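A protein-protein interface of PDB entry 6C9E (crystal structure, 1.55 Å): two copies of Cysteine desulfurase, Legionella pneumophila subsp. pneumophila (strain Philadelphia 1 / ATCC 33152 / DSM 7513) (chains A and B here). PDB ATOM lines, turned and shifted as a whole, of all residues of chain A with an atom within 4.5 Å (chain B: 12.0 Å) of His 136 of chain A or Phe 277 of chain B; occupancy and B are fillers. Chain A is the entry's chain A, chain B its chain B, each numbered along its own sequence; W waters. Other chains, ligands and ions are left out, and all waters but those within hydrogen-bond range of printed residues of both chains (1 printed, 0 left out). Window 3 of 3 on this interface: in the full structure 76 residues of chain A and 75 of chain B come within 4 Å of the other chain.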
ATOM      1  N   ILE A 134      16.781 -22.381  -6.378  1.00  0.00           N
ATOM      2  CA  ILE A 134      16.078 -22.882  -7.565  1.00  0.00           C
ATOM      3  C   ILE A 134      16.209 -21.830  -8.672  1.00  0.00           C
ATOM      4  O   ILE A 134      16.788 -20.767  -8.458  1.00  0.00           O
ATOM      5  CB  ILE A 134      14.596 -23.201  -7.272  1.00  0.00           C
ATOM      6  CG1 ILE A 134      13.847 -21.927  -6.855  1.00  0.00           C
ATOM      7  CG2 ILE A 134      14.493 -24.252  -6.165  1.00  0.00           C
ATOM      8  CD1 ILE A 134      12.328 -22.128  -6.745  1.00  0.00           C
ATOM      9  N   THR A 135      15.687 -22.136  -9.867  1.00  0.00           N
ATOM     10  CA  THR A 135      15.619 -21.127 -10.926  1.00  0.00           C
ATOM     11  C   THR A 135      14.217 -20.538 -11.042  1.00  0.00           C
ATOM     12  O   THR A 135      13.227 -21.094 -10.553  1.00  0.00           O
ATOM     13  CB  THR A 135      16.021 -21.662 -12.310  1.00  0.00           C
ATOM     14  OG1 THR A 135      14.935 -22.383 -12.896  1.00  0.00           O
ATOM     15  CG2 THR A 135      17.246 -22.568 -12.255  1.00  0.00           C
ATOM     16  N   HIS A 136      14.141 -19.396 -11.740  1.00  0.00           N
ATOM     17  CA  HIS A 136      12.846 -18.752 -11.943  1.00  0.00           C
ATOM     18  C   HIS A 136      11.900 -19.601 -12.774  1.00  0.00           C
ATOM     19  O   HIS A 136      10.687 -19.376 -12.726  1.00  0.00           O
ATOM     20  CB  HIS A 136      13.049 -17.391 -12.624  1.00  0.00           C
ATOM     21  CG  HIS A 136      12.005 -16.363 -12.288  1.00  0.00           C
ATOM     22  ND1 HIS A 136      12.304 -15.023 -12.172  1.00  0.00           N
ATOM     23  CD2 HIS A 136      10.666 -16.463 -12.105  1.00  0.00           C
ATOM     24  CE1 HIS A 136      11.203 -14.345 -11.898  1.00  0.00           C
ATOM     25  NE2 HIS A 136      10.195 -15.195 -11.841  1.00  0.00           N
ATOM     26  N   MET A 137      12.410 -20.534 -13.563  1.00  0.00           N
ATOM     27  CA  MET A 137      11.528 -21.251 -14.479  1.00  0.00           C
ATOM     28  C   MET A 137      11.008 -22.573 -13.924  1.00  0.00           C
ATOM     29  O   MET A 137      10.446 -23.371 -14.688  1.00  0.00           O
ATOM     30  CB  MET A 137      12.235 -21.492 -15.819  1.00  0.00           C
ATOM     31  CG  MET A 137      13.346 -22.544 -15.780  1.00  0.00           C
ATOM     32  SD  MET A 137      14.077 -22.833 -17.408  1.00  0.00           S
ATOM     33  CE  MET A 137      14.973 -21.294 -17.690  1.00  0.00           C
ATOM     34  N   GLU A 138      11.173 -22.839 -12.627  1.00  0.00           N
ATOM     35  CA  GLU A 138      10.736 -24.133 -12.106  1.00  0.00           C
ATOM     36  C   GLU A 138       9.231 -24.326 -12.254  1.00  0.00           C
ATOM     37  O   GLU A 138       8.431 -23.404 -12.079  1.00  0.00           O
ATOM     38  CB  GLU A 138      11.097 -24.292 -10.629  1.00  0.00           C
ATOM     39  CG  GLU A 138      12.569 -24.250 -10.268  1.00  0.00           C
ATOM     40  CD  GLU A 138      13.447 -25.113 -11.134  1.00  0.00           C
ATOM     41  OE1 GLU A 138      13.060 -26.275 -11.409  1.00  0.00           O
ATOM     42  OE2 GLU A 138      14.539 -24.621 -11.526  1.00  0.00           O
ATOM     43  N   ILE A 143       8.979 -26.184  -6.680  1.00  0.00           N
ATOM     44  CA  ILE A 143       8.913 -24.953  -5.890  1.00  0.00           C
ATOM     45  C   ILE A 143       8.259 -25.256  -4.552  1.00  0.00           C
ATOM     46  O   ILE A 143       8.849 -25.025  -3.495  1.00  0.00           O
ATOM     47  CB  ILE A 143       8.130 -23.833  -6.602  1.00  0.00           C
ATOM     48  CG1 ILE A 143       8.814 -23.450  -7.914  1.00  0.00           C
ATOM     49  CG2 ILE A 143       8.015 -22.605  -5.673  1.00  0.00           C
ATOM     50  CD1 ILE A 143       7.985 -22.434  -8.751  1.00  0.00           C
ATOM     51  N   GLN A 147       9.246 -24.654  -0.526  1.00  0.00           N
ATOM     52  CA  GLN A 147       8.551 -23.659   0.290  1.00  0.00           C
ATOM     53  C   GLN A 147       8.029 -24.269   1.582  1.00  0.00           C
ATOM     54  O   GLN A 147       8.036 -23.607   2.635  1.00  0.00           O
ATOM     55  CB  GLN A 147       7.394 -23.036  -0.487  1.00  0.00           C
ATOM     56  CG  GLN A 147       7.842 -22.174  -1.667  1.00  0.00           C
ATOM     57  CD  GLN A 147       6.661 -21.584  -2.401  1.00  0.00           C
ATOM     58  OE1 GLN A 147       5.660 -22.275  -2.609  1.00  0.00           O
ATOM     59  NE2 GLN A 147       6.763 -20.305  -2.792  1.00  0.00           N
ATOM     60  N   VAL A 159      16.120 -17.655  -5.620  1.00  0.00           N
ATOM     61  CA  VAL A 159      15.686 -17.902  -6.995  1.00  0.00           C
ATOM     62  C   VAL A 159      16.677 -17.260  -7.959  1.00  0.00           C
ATOM     63  O   VAL A 159      16.850 -16.037  -7.954  1.00  0.00           O
ATOM     64  CB  VAL A 159      14.269 -17.353  -7.257  1.00  0.00           C
ATOM     65  CG1 VAL A 159      13.830 -17.713  -8.668  1.00  0.00           C
ATOM     66  CG2 VAL A 159      13.281 -17.898  -6.228  1.00  0.00           C
ATOM     67  N   ALA A 160      17.282 -18.075  -8.810  1.00  0.00           N
ATOM     68  CA  ALA A 160      18.199 -17.586  -9.837  1.00  0.00           C
ATOM     69  C   ALA A 160      17.406 -17.048 -11.025  1.00  0.00           C
ATOM     70  O   ALA A 160      16.503 -17.732 -11.521  1.00  0.00           O
ATOM     71  CB  ALA A 160      19.124 -18.719 -10.295  1.00  0.00           C
ATOM     72  N   PRO A 161      17.737 -15.862 -11.527  1.00  0.00           N
ATOM     73  CA  PRO A 161      16.919 -15.228 -12.566  1.00  0.00           C
ATOM     74  C   PRO A 161      17.205 -15.777 -13.955  1.00  0.00           C
ATOM     75  O   PRO A 161      18.231 -16.413 -14.210  1.00  0.00           O
ATOM     76  CB  PRO A 161      17.334 -13.755 -12.482  1.00  0.00           C
ATOM     77  CG  PRO A 161      18.760 -13.807 -11.998  1.00  0.00           C
ATOM     78  CD  PRO A 161      18.803 -14.971 -11.030  1.00  0.00           C
ATOM     79  N   ILE A 162      16.264 -15.504 -14.864  1.00  0.00           N
ATOM     80  CA  ILE A 162      16.412 -15.822 -16.276  1.00  0.00           C
ATOM     81  C   ILE A 162      16.399 -14.525 -17.075  1.00  0.00           C
ATOM     82  O   ILE A 162      15.928 -13.474 -16.622  1.00  0.00           O
ATOM     83  CB  ILE A 162      15.315 -16.779 -16.790  1.00  0.00           C
ATOM     84  CG1 ILE A 162      13.944 -16.124 -16.677  1.00  0.00           C
ATOM     85  CG2 ILE A 162      15.340 -18.094 -15.996  1.00  0.00           C
ATOM     86  CD1 ILE A 162      12.893 -16.800 -17.509  1.00  0.00           C
ATOM     87  N   PRO A 383       5.237 -18.170 -11.555  1.00  0.00           N
ATOM     88  CA  PRO A 383       6.271 -17.127 -11.460  1.00  0.00           C
ATOM     89  C   PRO A 383       6.868 -16.757 -12.804  1.00  0.00           C
ATOM     90  O   PRO A 383       7.208 -15.585 -13.014  1.00  0.00           O
ATOM     91  CB  PRO A 383       7.300 -17.751 -10.510  1.00  0.00           C
ATOM     92  CG  PRO A 383       6.460 -18.691  -9.629  1.00  0.00           C
ATOM     93  CD  PRO A 383       5.514 -19.293 -10.636  1.00  0.00           C
ATOM     94  N   LEU A 384       6.955 -17.704 -13.741  1.00  0.00           N
ATOM     95  CA  LEU A 384       7.376 -17.373 -15.101  1.00  0.00           C
ATOM     96  C   LEU A 384       6.383 -16.455 -15.778  1.00  0.00           C
ATOM     97  O   LEU A 384       6.770 -15.526 -16.504  1.00  0.00           O
ATOM     98  CB  LEU A 384       7.499 -18.639 -15.946  1.00  0.00           C
ATOM     99  CG  LEU A 384       8.830 -19.344 -16.044  1.00  0.00           C
ATOM    100  CD1 LEU A 384       8.734 -20.451 -17.100  1.00  0.00           C
ATOM    101  CD2 LEU A 384       9.897 -18.336 -16.390  1.00  0.00           C
ATOM    102  N   PHE A 387       7.038 -13.085 -14.547  1.00  0.00           N
ATOM    103  CA  PHE A 387       8.247 -12.509 -15.146  1.00  0.00           C
ATOM    104  C   PHE A 387       7.979 -11.940 -16.536  1.00  0.00           C
ATOM    105  O   PHE A 387       8.462 -10.844 -16.873  1.00  0.00           O
ATOM    106  CB  PHE A 387       9.354 -13.566 -15.216  1.00  0.00           C
ATOM    107  CG  PHE A 387      10.607 -13.095 -15.938  1.00  0.00           C
ATOM    108  CD1 PHE A 387      11.454 -12.171 -15.357  1.00  0.00           C
ATOM    109  CD2 PHE A 387      10.918 -13.587 -17.193  1.00  0.00           C
ATOM    110  CE1 PHE A 387      12.608 -11.737 -16.013  1.00  0.00           C
ATOM    111  CE2 PHE A 387      12.062 -13.155 -17.866  1.00  0.00           C
ATOM    112  CZ  PHE A 387      12.907 -12.232 -17.269  1.00  0.00           C
ATOM    113  N   GLY B 268       3.096 -29.357  -4.719  1.00  0.00           N
ATOM    114  CA  GLY B 268       3.535 -29.168  -6.082  1.00  0.00           C
ATOM    115  C   GLY B 268       2.374 -28.759  -6.964  1.00  0.00           C
ATOM    116  O   GLY B 268       1.404 -28.158  -6.498  1.00  0.00           O
ATOM    117  N   ILE B 272      -2.325 -26.601  -5.723  1.00  0.00           N
ATOM    118  CA  ILE B 272      -2.298 -25.175  -5.415  1.00  0.00           C
ATOM    119  C   ILE B 272      -3.439 -24.464  -6.133  1.00  0.00           C
ATOM    120  O   ILE B 272      -3.946 -24.921  -7.163  1.00  0.00           O
ATOM    121  CB  ILE B 272      -0.948 -24.528  -5.806  1.00  0.00           C
ATOM    122  CG1 ILE B 272      -0.662 -24.638  -7.326  1.00  0.00           C
ATOM    123  CG2 ILE B 272       0.195 -25.132  -4.997  1.00  0.00           C
ATOM    124  CD1 ILE B 272      -1.109 -23.410  -8.167  1.00  0.00           C
ATOM    125  N   ASN B 273      -3.833 -23.308  -5.577  1.00  0.00           N
ATOM    126  CA  ASN B 273      -4.583 -22.283  -6.299  1.00  0.00           C
ATOM    127  C   ASN B 273      -3.651 -21.253  -6.927  1.00  0.00           C
ATOM    128  O   ASN B 273      -3.884 -20.800  -8.051  1.00  0.00           O
ATOM    129  CB  ASN B 273      -5.560 -21.560  -5.361  1.00  0.00           C
ATOM    130  CG  ASN B 273      -6.817 -22.372  -5.066  1.00  0.00           C
ATOM    131  OD1 ASN B 273      -7.139 -23.324  -5.779  1.00  0.00           O
ATOM    132  ND2 ASN B 273      -7.544 -21.976  -4.012  1.00  0.00           N
ATOM    133  N   SER B 274      -2.600 -20.861  -6.217  1.00  0.00           N
ATOM    134  CA  SER B 274      -1.672 -19.860  -6.718  1.00  0.00           C
ATOM    135  C   SER B 274      -0.302 -20.101  -6.103  1.00  0.00           C
ATOM    136  O   SER B 274      -0.209 -20.460  -4.925  1.00  0.00           O
ATOM    137  CB  SER B 274      -2.178 -18.454  -6.380  1.00  0.00           C
ATOM    138  OG  SER B 274      -1.284 -17.456  -6.827  1.00  0.00           O
ATOM    139  N   VAL B 275       0.751 -19.892  -6.896  1.00  0.00           N
ATOM    140  CA  VAL B 275       2.131 -19.990  -6.427  1.00  0.00           C
ATOM    141  C   VAL B 275       2.850 -18.701  -6.793  1.00  0.00           C
ATOM    142  O   VAL B 275       2.887 -18.311  -7.968  1.00  0.00           O
ATOM    143  CB  VAL B 275       2.869 -21.195  -7.043  1.00  0.00           C
ATOM    144  CG1 VAL B 275       4.390 -21.096  -6.736  1.00  0.00           C
ATOM    145  CG2 VAL B 275       2.294 -22.503  -6.569  1.00  0.00           C
ATOM    146  N   SER B 276       3.414 -18.029  -5.795  1.00  0.00           N
ATOM    147  CA  SER B 276       4.413 -17.002  -6.029  1.00  0.00           C
ATOM    148  C   SER B 276       5.546 -17.246  -5.054  1.00  0.00           C
ATOM    149  O   SER B 276       5.467 -18.124  -4.198  1.00  0.00           O
ATOM    150  CB  SER B 276       3.846 -15.587  -5.863  1.00  0.00           C
ATOM    151  OG  SER B 276       3.752 -15.251  -4.498  1.00  0.00           O
ATOM    152  N   PHE B 277       6.613 -16.465  -5.181  1.00  0.00           N
ATOM    153  CA  PHE B 277       7.682 -16.602  -4.205  1.00  0.00           C
ATOM    154  C   PHE B 277       7.371 -15.868  -2.908  1.00  0.00           C
ATOM    155  O   PHE B 277       8.105 -16.030  -1.930  1.00  0.00           O
ATOM    156  CB  PHE B 277       9.000 -16.150  -4.848  1.00  0.00           C
ATOM    157  CG  PHE B 277       9.399 -17.018  -6.018  1.00  0.00           C
ATOM    158  CD1 PHE B 277       9.376 -18.397  -5.899  1.00  0.00           C
ATOM    159  CD2 PHE B 277       9.752 -16.463  -7.243  1.00  0.00           C
ATOM    160  CE1 PHE B 277       9.711 -19.212  -6.969  1.00  0.00           C
ATOM    161  CE2 PHE B 277      10.083 -17.280  -8.324  1.00  0.00           C
ATOM    162  CZ  PHE B 277      10.056 -18.655  -8.181  1.00  0.00           C
ATOM    163  N   GLU B 278       6.273 -15.105  -2.859  1.00  0.00           N
ATOM    164  CA  GLU B 278       5.859 -14.424  -1.641  1.00  0.00           C
ATOM    165  C   GLU B 278       4.731 -15.136  -0.905  1.00  0.00           C
ATOM    166  O   GLU B 278       4.592 -14.950   0.310  1.00  0.00           O
ATOM    167  CB  GLU B 278       5.419 -12.988  -1.958  1.00  0.00           C
ATOM    168  CG  GLU B 278       6.515 -12.141  -2.575  1.00  0.00           C
ATOM    169  CD  GLU B 278       7.693 -11.951  -1.635  1.00  0.00           C
ATOM    170  OE1 GLU B 278       7.474 -11.895  -0.403  1.00  0.00           O
ATOM    171  OE2 GLU B 278       8.837 -11.865  -2.128  1.00  0.00           O
ATOM    172  N   ALA B 279       3.934 -15.944  -1.600  1.00  0.00           N
ATOM    173  CA  ALA B 279       2.796 -16.607  -0.985  1.00  0.00           C
ATOM    174  C   ALA B 279       2.365 -17.757  -1.888  1.00  0.00           C
ATOM    175  O   ALA B 279       2.340 -17.608  -3.109  1.00  0.00           O
ATOM    176  CB  ALA B 279       1.633 -15.627  -0.780  1.00  0.00           C
ATOM    177  N   THR B 280       2.015 -18.889  -1.288  1.00  0.00           N
ATOM    178  CA  THR B 280       1.372 -19.979  -2.009  1.00  0.00           C
ATOM    179  C   THR B 280       0.047 -20.266  -1.331  1.00  0.00           C
ATOM    180  O   THR B 280      -0.001 -20.415  -0.102  1.00  0.00           O
ATOM    181  CB  THR B 280       2.240 -21.240  -2.047  1.00  0.00           C
ATOM    182  OG1 THR B 280       3.348 -21.010  -2.926  1.00  0.00           O
ATOM    183  CG2 THR B 280       1.447 -22.415  -2.588  1.00  0.00           C
ATOM    184  N   GLU B 281      -1.020 -20.323  -2.126  1.00  0.00           N
ATOM    185  CA  GLU B 281      -2.355 -20.655  -1.649  1.00  0.00           C
ATOM    186  C   GLU B 281      -2.745 -22.022  -2.177  1.00  0.00           C
ATOM    187  O   GLU B 281      -2.599 -22.289  -3.374  1.00  0.00           O
ATOM    188  CB  GLU B 281      -3.380 -19.624  -2.114  1.00  0.00           C
ATOM    189  CG  GLU B 281      -2.905 -18.178  -2.003  1.00  0.00           C
ATOM    190  CD  GLU B 281      -2.624 -17.750  -0.577  1.00  0.00           C
ATOM    191  OE1 GLU B 281      -3.210 -18.343   0.357  1.00  0.00           O
ATOM    192  OE2 GLU B 281      -1.816 -16.810  -0.393  1.00  0.00           O
ATOM    193  N   TYR B 282      -3.263 -22.874  -1.298  1.00  0.00           N
ATOM    194  CA  TYR B 282      -3.535 -24.247  -1.682  1.00  0.00           C
ATOM    195  C   TYR B 282      -4.967 -24.417  -2.183  1.00  0.00           C
ATOM    196  O   TYR B 282      -5.867 -23.619  -1.884  1.00  0.00           O
ATOM    197  CB  TYR B 282      -3.264 -25.196  -0.511  1.00  0.00           C
ATOM    198  CG  TYR B 282      -1.807 -25.187  -0.130  1.00  0.00           C
ATOM    199  CD1 TYR B 282      -1.379 -24.691   1.094  1.00  0.00           C
ATOM    200  CD2 TYR B 282      -0.851 -25.644  -1.028  1.00  0.00           C
ATOM    201  CE1 TYR B 282      -0.034 -24.664   1.419  1.00  0.00           C
ATOM    202  CE2 TYR B 282       0.486 -25.629  -0.710  1.00  0.00           C
ATOM    203  CZ  TYR B 282       0.893 -25.145   0.514  1.00  0.00           C
ATOM    204  OH  TYR B 282       2.242 -25.134   0.813  1.00  0.00           O
HETATM  205  O   HOH W   1       8.953 -18.686  -1.839  1.00  0.00           O
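No position is printed for both chains.
Printed residues of chain B that touch a printed residue of chain A: Val 275, Ser 276, Phe 277 and Thr 280.
Among the printed residues, 7 pairs touch across the chains.
Among the printed residues, no Asp or Glu carboxylate lies within 4 Å of a Lys or Arg side-chain nitrogen of the other chain.
The backbone carbonyl oxygen (O) of Ser 276 of chain B sits at hydrogen-bond distance from the side-chain amide nitrogen (NE2) of Gln 147 of chain A, at 2.9 Å.
The side-chain amide oxygen of Gln 147 of chain A lies within hydrogen-bond range of the side-chain hydroxyl of Thr 280 of chain B.
The backbone NH of Ala 160 of chain A lies within hydrogen-bond range of the backbone carbonyl oxygen of Ile 134 of chain A, 2.8 Å away.
The backbone NH (N) of His 136 of chain A lies within hydrogen-bond range of the backbone carbonyl oxygen (O) of Ala 160 of chain A, at 2.9 Å.
The backbone carbonyl oxygen (O) of Pro 383 of chain A lies within hydrogen-bond range of a ring nitrogen (NE2) of His 136 of chain A (3.2 Å).
The backbone NH of Glu 278 of chain B is in hydrogen-bond range of the side-chain hydroxyl of Ser 276 of chain B.
The side-chain hydroxyl (OG) of Ser 276 of chain B lies within hydrogen-bond range of the backbone NH (N) of Ala 279 of chain B, 3.0 Å away.
Water W1 lies within hydrogen-bond range of the backbone carbonyl oxygen (O) of Phe 277 of chain B and the side-chain amide nitrogen (NE2) of Gln 147 of chain A.
His 136 of chain A touches one residue of chain B.
Of the printed residues of chain A, Phe 277 of chain B touches Ile 134 (3.9 Å), His 136 (3.9 Å), Val 159 (3.8 Å) and Pro 383 (3.6 Å).
Thr 135 of chain A touches none of the printed residues of chain B.
No residue of chain B comes within 4 Å of Met 137 of chain A.
No residue of chain B comes within 4 Å of Glu 138 of chain A.
Of chain B, only Phe 277 comes within 4 Å of Val 159 of chain A.
No residue of chain B comes within 4 Å of Ala 160 of chain A.
Pro 161 of chain A touches none of the printed residues of chain B.
No residue of chain B comes within 4 Å of Ile 162 of chain A.
Of chain B, only Val 275 (3.9 Å) and Phe 277 (3.6 Å) come within 4 Å of Pro 383 of chain A.
Printed residues of chain A within 4 Å of Ser 276 of chain B: Gln 147.
Of the printed residues of chain A, Thr 280 of chain B touches Gln 147 (2.7 Å).
Of the printed residues of chain B, Gln 147 of chain A touches Ser 276 (2.9 Å) and Thr 280 (2.7 Å).
Of the printed residues of chain A, Val 275 of chain B touches Pro 383 (3.9 Å).
Asn 273 of chain B touches none of the printed residues of chain A.
The nearest printed residue of chain A that does not touch Ser 276 of chain B is Pro 383 of chain A (4.5 Å).
Phe 277 of chain B touches Ile 134 of chain A.
His 136 of chain A touches Phe 277 of chain B.
CG1 of Val 159 of chain A touches CE2 of Phe 277 of chain B, at 3.8 Å.
Pro 383 of chain A touches Val 275 of chain B.
Pro 383 of chain A touches Phe 277 of chain B (CB to CE2, 3.6 Å).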
